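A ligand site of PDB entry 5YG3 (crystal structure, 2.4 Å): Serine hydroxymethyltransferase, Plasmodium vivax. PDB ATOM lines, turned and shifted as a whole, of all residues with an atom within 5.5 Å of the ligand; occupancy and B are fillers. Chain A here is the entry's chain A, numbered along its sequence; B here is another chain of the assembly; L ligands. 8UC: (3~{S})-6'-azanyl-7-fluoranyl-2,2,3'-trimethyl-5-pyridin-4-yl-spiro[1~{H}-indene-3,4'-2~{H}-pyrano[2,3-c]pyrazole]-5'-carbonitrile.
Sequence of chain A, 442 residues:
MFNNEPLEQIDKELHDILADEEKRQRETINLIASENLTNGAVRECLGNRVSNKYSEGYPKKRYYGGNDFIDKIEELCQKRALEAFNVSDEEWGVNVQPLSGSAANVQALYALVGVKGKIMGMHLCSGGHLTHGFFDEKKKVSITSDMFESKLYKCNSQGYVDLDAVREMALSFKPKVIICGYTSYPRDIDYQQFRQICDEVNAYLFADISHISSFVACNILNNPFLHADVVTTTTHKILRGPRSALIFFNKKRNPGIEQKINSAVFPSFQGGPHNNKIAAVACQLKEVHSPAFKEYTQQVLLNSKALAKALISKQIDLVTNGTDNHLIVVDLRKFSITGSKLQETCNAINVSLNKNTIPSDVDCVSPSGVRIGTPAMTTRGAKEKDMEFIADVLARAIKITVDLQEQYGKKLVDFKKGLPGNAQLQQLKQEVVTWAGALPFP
The backbone carbonyl oxygen (O) of Gly 128 sits at hydrogen-bond distance from a nitrogen (N7) of the ligand, 3.0 Å away.
O of Leu 124 lies within hydrogen-bond range of N7 of the ligand, at 3.2 Å.
N12 of the ligand lies close to NE2 of His 129, 3.2 Å away.
The side-chain hydroxyl of Thr 183 sits at hydrogen-bond distance from an oxygen (O1) of the ligand (3.0 Å).
The backbone NH (N) of Tyr 63 of chain B sits at hydrogen-bond distance from the backbone carbonyl oxygen (O) of Glu 56 of chain B, 3.3 Å away.
O of Thr 183 is in hydrogen-bond range of NH1 of Arg 371, at 3.0 Å.
The backbone carbonyl oxygen of Asn 354 sits at hydrogen-bond distance from the backbone NH of Arg 371, at 2.8 Å.
The backbone carbonyl oxygen (O) of Gly 127 is in hydrogen-bond range of the backbone NH (N) of Ser 184 (3.0 Å).
The side-chain hydroxyl (OG1) of Thr 357 sits at hydrogen-bond distance from the backbone carbonyl oxygen (O) of Cys 125, at 2.5 Å.
O of Gly 127 is in hydrogen-bond range of N of Thr 183.
OH of Tyr 64 of chain B lies within hydrogen-bond range of NH2 of Arg 371, 3.3 Å away.
Merely in contact with the ligand: Tyr 64 of chain B (3.0 Å), Leu 130 (3.2 Å), Tyr 63 of chain B (3.2 Å), Glu 56 of chain B (3.3 Å), Lys 355 (3.5 Å), Asn 354 (3.8 Å), Thr 357 (3.9 Å), Cys 364 (3.9 Å) and Gly 127 (3.95 Å).
Hydrophobic or aromatic side chains that line the ligand: Leu 124, His 129, Leu 130, Tyr 63 of chain B and Tyr 64 of chain B.
Within 4 Å of the ligand: Leu 124, Gly 127, Gly 128, His 129, Leu 130, Thr 183, Asn 354, Lys 355, Thr 357, Cys 364, Glu 56 of chain B, Tyr 63 of chain B and Tyr 64 of chain B.
Along chain A the residues within 4 Å of the ligand span positions 124 to 364.
The nearest printed residue that does not touch the ligand is Arg 371 (4.1 Å).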
ATOM      1  N   LEU A 124     -30.219   7.586  -1.985  1.00  0.00           N
ATOM      2  CA  LEU A 124     -29.668   6.651  -0.986  1.00  0.00           C
ATOM      3  C   LEU A 124     -29.931   5.204  -1.373  1.00  0.00           C
ATOM      4  O   LEU A 124     -29.000   4.405  -1.446  1.00  0.00           O
ATOM      5  CB  LEU A 124     -30.291   6.941   0.377  1.00  0.00           C
ATOM      6  CG  LEU A 124     -29.896   6.081   1.586  1.00  0.00           C
ATOM      7  CD1 LEU A 124     -28.620   6.627   2.212  1.00  0.00           C
ATOM      8  CD2 LEU A 124     -31.043   6.043   2.595  1.00  0.00           C
ATOM      9  N   CYS A 125     -31.205   4.864  -1.573  1.00  0.00           N
ATOM     10  CA  CYS A 125     -31.644   3.585  -2.156  1.00  0.00           C
ATOM     11  C   CYS A 125     -30.834   3.096  -3.369  1.00  0.00           C
ATOM     12  O   CYS A 125     -30.543   1.901  -3.465  1.00  0.00           O
ATOM     13  CB  CYS A 125     -33.143   3.658  -2.506  1.00  0.00           C
ATOM     14  SG  CYS A 125     -34.258   3.787  -1.054  1.00  0.00           S
ATOM     15  N   GLY A 127     -27.670   4.057  -4.128  1.00  0.00           N
ATOM     16  CA  GLY A 127     -26.242   3.892  -3.801  1.00  0.00           C
ATOM     17  C   GLY A 127     -25.472   5.121  -3.380  1.00  0.00           C
ATOM     18  O   GLY A 127     -24.286   5.024  -3.137  1.00  0.00           O
ATOM     19  N   GLY A 128     -26.120   6.279  -3.296  1.00  0.00           N
ATOM     20  CA  GLY A 128     -25.489   7.499  -2.826  1.00  0.00           C
ATOM     21  C   GLY A 128     -25.510   7.704  -1.303  1.00  0.00           C
ATOM     22  O   GLY A 128     -26.190   6.957  -0.541  1.00  0.00           O
ATOM     23  N   HIS A 129     -24.748   8.708  -0.851  1.00  0.00           N
ATOM     24  CA  HIS A 129     -24.662   9.018   0.572  1.00  0.00           C
ATOM     25  C   HIS A 129     -25.745   9.965   1.055  1.00  0.00           C
ATOM     26  O   HIS A 129     -26.364  10.685   0.274  1.00  0.00           O
ATOM     27  CB  HIS A 129     -23.270   9.564   0.946  1.00  0.00           C
ATOM     28  CG  HIS A 129     -22.920   9.318   2.369  1.00  0.00           C
ATOM     29  ND1 HIS A 129     -22.774  10.334   3.282  1.00  0.00           N
ATOM     30  CD2 HIS A 129     -22.763   8.168   3.055  1.00  0.00           C
ATOM     31  CE1 HIS A 129     -22.522   9.816   4.473  1.00  0.00           C
ATOM     32  NE2 HIS A 129     -22.489   8.507   4.354  1.00  0.00           N
ATOM     33  N   LEU A 130     -25.976   9.938   2.374  1.00  0.00           N
ATOM     34  CA  LEU A 130     -26.912  10.855   3.062  1.00  0.00           C
ATOM     35  C   LEU A 130     -26.565  12.302   2.777  1.00  0.00           C
ATOM     36  O   LEU A 130     -27.443  13.132   2.490  1.00  0.00           O
ATOM     37  CB  LEU A 130     -26.871  10.629   4.579  1.00  0.00           C
ATOM     38  CG  LEU A 130     -27.419   9.278   5.066  1.00  0.00           C
ATOM     39  CD1 LEU A 130     -26.961   9.042   6.485  1.00  0.00           C
ATOM     40  CD2 LEU A 130     -28.942   9.242   4.999  1.00  0.00           C
ATOM     41  N   PHE A 134     -29.847  13.587   0.685  1.00  0.00           N
ATOM     42  CA  PHE A 134     -30.894  12.612   0.978  1.00  0.00           C
ATOM     43  C   PHE A 134     -32.017  13.175   1.838  1.00  0.00           C
ATOM     44  O   PHE A 134     -31.754  13.672   2.922  1.00  0.00           O
ATOM     45  CB  PHE A 134     -30.379  11.366   1.705  1.00  0.00           C
ATOM     46  CG  PHE A 134     -31.497  10.435   2.053  1.00  0.00           C
ATOM     47  CD1 PHE A 134     -32.195   9.757   1.045  1.00  0.00           C
ATOM     48  CD2 PHE A 134     -31.946  10.349   3.364  1.00  0.00           C
ATOM     49  CE1 PHE A 134     -33.294   8.949   1.351  1.00  0.00           C
ATOM     50  CE2 PHE A 134     -33.044   9.543   3.684  1.00  0.00           C
ATOM     51  CZ  PHE A 134     -33.714   8.856   2.676  1.00  0.00           C
ATOM     52  N   VAL A 141     -34.045  14.401   5.978  1.00  0.00           N
ATOM     53  CA  VAL A 141     -33.204  13.551   6.830  1.00  0.00           C
ATOM     54  C   VAL A 141     -31.752  14.054   6.929  1.00  0.00           C
ATOM     55  O   VAL A 141     -31.136  13.950   7.987  1.00  0.00           O
ATOM     56  CB  VAL A 141     -33.279  12.067   6.385  1.00  0.00           C
ATOM     57  CG1 VAL A 141     -32.275  11.173   7.115  1.00  0.00           C
ATOM     58  CG2 VAL A 141     -34.700  11.531   6.601  1.00  0.00           C
ATOM     59  N   THR A 183     -21.606   5.496  -2.108  1.00  0.00           N
ATOM     60  CA  THR A 183     -21.440   4.672  -0.902  1.00  0.00           C
ATOM     61  C   THR A 183     -21.570   3.182  -1.224  1.00  0.00           C
ATOM     62  O   THR A 183     -20.775   2.386  -0.739  1.00  0.00           O
ATOM     63  CB  THR A 183     -22.301   5.104   0.318  1.00  0.00           C
ATOM     64  OG1 THR A 183     -23.029   3.980   0.859  1.00  0.00           O
ATOM     65  CG2 THR A 183     -23.244   6.159  -0.004  1.00  0.00           C
ATOM     66  N   SER A 184     -22.532   2.795  -2.063  1.00  0.00           N
ATOM     67  CA  SER A 184     -22.632   1.399  -2.460  1.00  0.00           C
ATOM     68  C   SER A 184     -22.924   1.234  -3.913  1.00  0.00           C
ATOM     69  O   SER A 184     -23.922   0.673  -4.291  1.00  0.00           O
ATOM     70  CB  SER A 184     -23.664   0.671  -1.603  1.00  0.00           C
ATOM     71  OG  SER A 184     -24.972   0.911  -2.048  1.00  0.00           O
ATOM     72  N   ASN A 354     -23.435  -5.810   5.683  1.00  0.00           N
ATOM     73  CA  ASN A 354     -24.587  -4.979   5.996  1.00  0.00           C
ATOM     74  C   ASN A 354     -25.669  -5.084   4.946  1.00  0.00           C
ATOM     75  O   ASN A 354     -25.400  -5.459   3.803  1.00  0.00           O
ATOM     76  CB  ASN A 354     -24.177  -3.530   6.292  1.00  0.00           C
ATOM     77  CG  ASN A 354     -23.625  -2.794   5.079  1.00  0.00           C
ATOM     78  OD1 ASN A 354     -22.418  -2.764   4.873  1.00  0.00           O
ATOM     79  ND2 ASN A 354     -24.518  -2.207   4.271  1.00  0.00           N
ATOM     80  N   LYS A 355     -26.889  -4.791   5.396  1.00  0.00           N
ATOM     81  CA  LYS A 355     -28.054  -4.795   4.531  1.00  0.00           C
ATOM     82  C   LYS A 355     -27.987  -3.604   3.585  1.00  0.00           C
ATOM     83  O   LYS A 355     -27.436  -2.567   3.934  1.00  0.00           O
ATOM     84  CB  LYS A 355     -29.379  -4.765   5.318  1.00  0.00           C
ATOM     85  CG  LYS A 355     -29.470  -3.733   6.428  1.00  0.00           C
ATOM     86  CD  LYS A 355     -30.887  -3.435   6.898  1.00  0.00           C
ATOM     87  CE  LYS A 355     -30.882  -2.560   8.143  1.00  0.00           C
ATOM     88  NZ  LYS A 355     -32.237  -2.459   8.760  1.00  0.00           N
ATOM     89  N   ASN A 356     -28.585  -3.773   2.413  1.00  0.00           N
ATOM     90  CA  ASN A 356     -28.464  -2.838   1.335  1.00  0.00           C
ATOM     91  C   ASN A 356     -29.649  -2.969   0.356  1.00  0.00           C
ATOM     92  O   ASN A 356     -30.005  -4.084  -0.069  1.00  0.00           O
ATOM     93  CB  ASN A 356     -27.118  -3.099   0.608  1.00  0.00           C
ATOM     94  CG  ASN A 356     -26.611  -1.877  -0.142  1.00  0.00           C
ATOM     95  OD1 ASN A 356     -25.629  -1.265   0.245  1.00  0.00           O
ATOM     96  ND2 ASN A 356     -27.296  -1.528  -1.210  1.00  0.00           N
ATOM     97  N   THR A 357     -30.264  -1.841   0.015  1.00  0.00           N
ATOM     98  CA  THR A 357     -31.365  -1.809  -0.948  1.00  0.00           C
ATOM     99  C   THR A 357     -30.908  -2.222  -2.342  1.00  0.00           C
ATOM    100  O   THR A 357     -29.709  -2.251  -2.634  1.00  0.00           O
ATOM    101  CB  THR A 357     -31.974  -0.396  -1.071  1.00  0.00           C
ATOM    102  OG1 THR A 357     -30.930   0.536  -1.359  1.00  0.00           O
ATOM    103  CG2 THR A 357     -32.677   0.036   0.201  1.00  0.00           C
ATOM    104  N   CYS A 364     -36.559   1.956   1.868  1.00  0.00           N
ATOM    105  CA  CYS A 364     -35.448   1.427   2.684  1.00  0.00           C
ATOM    106  C   CYS A 364     -35.812   0.557   3.905  1.00  0.00           C
ATOM    107  O   CYS A 364     -34.906   0.078   4.595  1.00  0.00           O
ATOM    108  CB  CYS A 364     -34.545   2.581   3.145  1.00  0.00           C
ATOM    109  SG  CYS A 364     -33.573   3.382   1.855  1.00  0.00           S
ATOM    110  N   PRO A 367     -34.678  -3.747   3.027  1.00  0.00           N
ATOM    111  CA  PRO A 367     -33.871  -3.789   1.796  1.00  0.00           C
ATOM    112  C   PRO A 367     -33.545  -5.201   1.337  1.00  0.00           C
ATOM    113  O   PRO A 367     -33.222  -6.059   2.171  1.00  0.00           O
ATOM    114  CB  PRO A 367     -32.587  -3.055   2.197  1.00  0.00           C
ATOM    115  CG  PRO A 367     -32.505  -3.189   3.652  1.00  0.00           C
ATOM    116  CD  PRO A 367     -33.921  -3.150   4.142  1.00  0.00           C
ATOM    117  N   ARG A 371     -24.457  -5.708   1.167  1.00  0.00           N
ATOM    118  CA  ARG A 371     -23.226  -5.241   0.608  1.00  0.00           C
ATOM    119  C   ARG A 371     -22.009  -5.899   1.250  1.00  0.00           C
ATOM    120  O   ARG A 371     -21.939  -6.004   2.468  1.00  0.00           O
ATOM    121  CB  ARG A 371     -23.123  -3.736   0.794  1.00  0.00           C
ATOM    122  CG  ARG A 371     -21.952  -3.098   0.056  1.00  0.00           C
ATOM    123  CD  ARG A 371     -21.835  -1.648   0.447  1.00  0.00           C
ATOM    124  NE  ARG A 371     -21.557  -1.461   1.862  1.00  0.00           N
ATOM    125  CZ  ARG A 371     -21.356  -0.272   2.434  1.00  0.00           C
ATOM    126  NH1 ARG A 371     -21.399   0.838   1.707  1.00  0.00           N
ATOM    127  NH2 ARG A 371     -21.113  -0.198   3.742  1.00  0.00           N
ATOM    128  N   GLU B  56     -22.817   3.605  12.900  1.00  0.00           N
ATOM    129  CA  GLU B  56     -23.841   4.605  12.643  1.00  0.00           C
ATOM    130  C   GLU B  56     -25.130   4.289  13.380  1.00  0.00           C
ATOM    131  O   GLU B  56     -25.577   3.151  13.415  1.00  0.00           O
ATOM    132  CB  GLU B  56     -24.133   4.705  11.148  1.00  0.00           C
ATOM    133  CG  GLU B  56     -23.011   5.355  10.381  1.00  0.00           C
ATOM    134  CD  GLU B  56     -23.288   5.467   8.913  1.00  0.00           C
ATOM    135  OE1 GLU B  56     -23.538   4.421   8.284  1.00  0.00           O
ATOM    136  OE2 GLU B  56     -23.259   6.608   8.393  1.00  0.00           O
ATOM    137  N   TYR B  63     -27.444   0.594  12.557  1.00  0.00           N
ATOM    138  CA  TYR B  63     -27.653   0.065  11.218  1.00  0.00           C
ATOM    139  C   TYR B  63     -26.887  -1.250  11.005  1.00  0.00           C
ATOM    140  O   TYR B  63     -27.445  -2.177  10.431  1.00  0.00           O
ATOM    141  CB  TYR B  63     -27.302   1.127  10.142  1.00  0.00           C
ATOM    142  CG  TYR B  63     -28.379   2.190  10.086  1.00  0.00           C
ATOM    143  CD1 TYR B  63     -29.491   2.025   9.264  1.00  0.00           C
ATOM    144  CD2 TYR B  63     -28.328   3.306  10.898  1.00  0.00           C
ATOM    145  CE1 TYR B  63     -30.510   2.975   9.240  1.00  0.00           C
ATOM    146  CE2 TYR B  63     -29.335   4.261  10.880  1.00  0.00           C
ATOM    147  CZ  TYR B  63     -30.417   4.092  10.051  1.00  0.00           C
ATOM    148  OH  TYR B  63     -31.418   5.032  10.048  1.00  0.00           O
ATOM    149  N   TYR B  64     -25.633  -1.330  11.457  1.00  0.00           N
ATOM    150  CA  TYR B  64     -24.847  -2.583  11.322  1.00  0.00           C
ATOM    151  C   TYR B  64     -24.771  -3.361  12.618  1.00  0.00           C
ATOM    152  O   TYR B  64     -24.933  -2.812  13.689  1.00  0.00           O
ATOM    153  CB  TYR B  64     -23.410  -2.329  10.843  1.00  0.00           C
ATOM    154  CG  TYR B  64     -23.269  -1.431   9.640  1.00  0.00           C
ATOM    155  CD1 TYR B  64     -24.352  -1.112   8.824  1.00  0.00           C
ATOM    156  CD2 TYR B  64     -21.998  -0.907   9.288  1.00  0.00           C
ATOM    157  CE1 TYR B  64     -24.194  -0.294   7.744  1.00  0.00           C
ATOM    158  CE2 TYR B  64     -21.830  -0.088   8.186  1.00  0.00           C
ATOM    159  CZ  TYR B  64     -22.949   0.218   7.414  1.00  0.00           C
ATOM    160  OH  TYR B  64     -22.822   1.036   6.314  1.00  0.00           O
ATOM    161  N   PHE B 266     -26.854  12.690  14.149  1.00  0.00           N
ATOM    162  CA  PHE B 266     -26.911  11.687  13.076  1.00  0.00           C
ATOM    163  C   PHE B 266     -28.349  11.326  12.820  1.00  0.00           C
ATOM    164  O   PHE B 266     -29.030  10.974  13.768  1.00  0.00           O
ATOM    165  CB  PHE B 266     -26.146  10.405  13.464  1.00  0.00           C
ATOM    166  CG  PHE B 266     -26.402   9.236  12.536  1.00  0.00           C
ATOM    167  CD1 PHE B 266     -25.723   9.123  11.309  1.00  0.00           C
ATOM    168  CD2 PHE B 266     -27.295   8.218  12.886  1.00  0.00           C
ATOM    169  CE1 PHE B 266     -25.947   8.058  10.454  1.00  0.00           C
ATOM    170  CE2 PHE B 266     -27.520   7.152  12.031  1.00  0.00           C
ATOM    171  CZ  PHE B 266     -26.831   7.068  10.815  1.00  0.00           C
ATOM    172  N   PRO B 267     -28.820  11.325  11.576  1.00  0.00           N
ATOM    173  CA  PRO B 267     -28.018  11.496  10.365  1.00  0.00           C
ATOM    174  C   PRO B 267     -28.009  12.903   9.775  1.00  0.00           C
ATOM    175  O   PRO B 267     -27.509  13.083   8.651  1.00  0.00           O
ATOM    176  CB  PRO B 267     -28.670  10.506   9.374  1.00  0.00           C
ATOM    177  CG  PRO B 267     -29.982  10.115   9.984  1.00  0.00           C
ATOM    178  CD  PRO B 267     -30.185  10.865  11.249  1.00  0.00           C
HETATM  179  C2  8UC L   1     -26.275   4.074   1.673  1.00  0.00           C
HETATM  180  C3  8UC L   1     -26.980   3.220   2.476  1.00  0.00           C
HETATM  181  C4  8UC L   1     -26.848   3.276   4.024  1.00  0.00           C
HETATM  182  C5  8UC L   1     -26.225   4.571   4.486  1.00  0.00           C
HETATM  183  C6  8UC L   1     -25.516   5.470   3.564  1.00  0.00           C
HETATM  184  N9  8UC L   1     -28.378   1.535   1.348  1.00  0.00           N
HETATM  185  C10 8UC L   1     -26.108   5.335   5.789  1.00  0.00           C
HETATM  186  N12 8UC L   1     -25.016   6.579   4.135  1.00  0.00           N
HETATM  187  C13 8UC L   1     -26.614   5.040   7.195  1.00  0.00           C
HETATM  188  C17 8UC L   1     -28.387   1.750   4.982  1.00  0.00           C
HETATM  189  C19 8UC L   1     -30.290   3.650   5.747  1.00  0.00           C
HETATM  190  C35 8UC L   1     -30.499   2.275   6.005  1.00  0.00           C
HETATM  191  C38 8UC L   1     -27.228   0.909   4.535  1.00  0.00           C
HETATM  192  C41 8UC L   1     -31.278   4.700   6.151  1.00  0.00           C
HETATM  193  F29 8UC L   1     -29.703   0.001   5.849  1.00  0.00           F
HETATM  194  C18 8UC L   1     -29.542   1.327   5.619  1.00  0.00           C
HETATM  195  C14 8UC L   1     -26.095   1.990   4.484  1.00  0.00           C
HETATM  196  C30 8UC L   1     -25.524   2.203   5.901  1.00  0.00           C
HETATM  197  C15 8UC L   1     -24.944   1.480   3.582  1.00  0.00           C
HETATM  198  C46 8UC L   1     -32.623   4.660   5.765  1.00  0.00           C
HETATM  199  C45 8UC L   1     -33.494   5.682   6.191  1.00  0.00           C
HETATM  200  N44 8UC L   1     -33.042   6.703   6.965  1.00  0.00           N
HETATM  201  C43 8UC L   1     -31.749   6.777   7.363  1.00  0.00           C
HETATM  202  C42 8UC L   1     -30.853   5.770   6.957  1.00  0.00           C
HETATM  203  C20 8UC L   1     -29.114   4.043   5.105  1.00  0.00           C
HETATM  204  C16 8UC L   1     -28.175   3.071   4.722  1.00  0.00           C
HETATM  205  C8  8UC L   1     -27.704   2.331   1.889  1.00  0.00           C
HETATM  206  N7  8UC L   1     -26.358   4.041   0.320  1.00  0.00           N
HETATM  207  N11 8UC L   1     -25.398   6.439   5.485  1.00  0.00           N
HETATM  208  O1  8UC L   1     -25.409   5.110   2.240  1.00  0.00           O
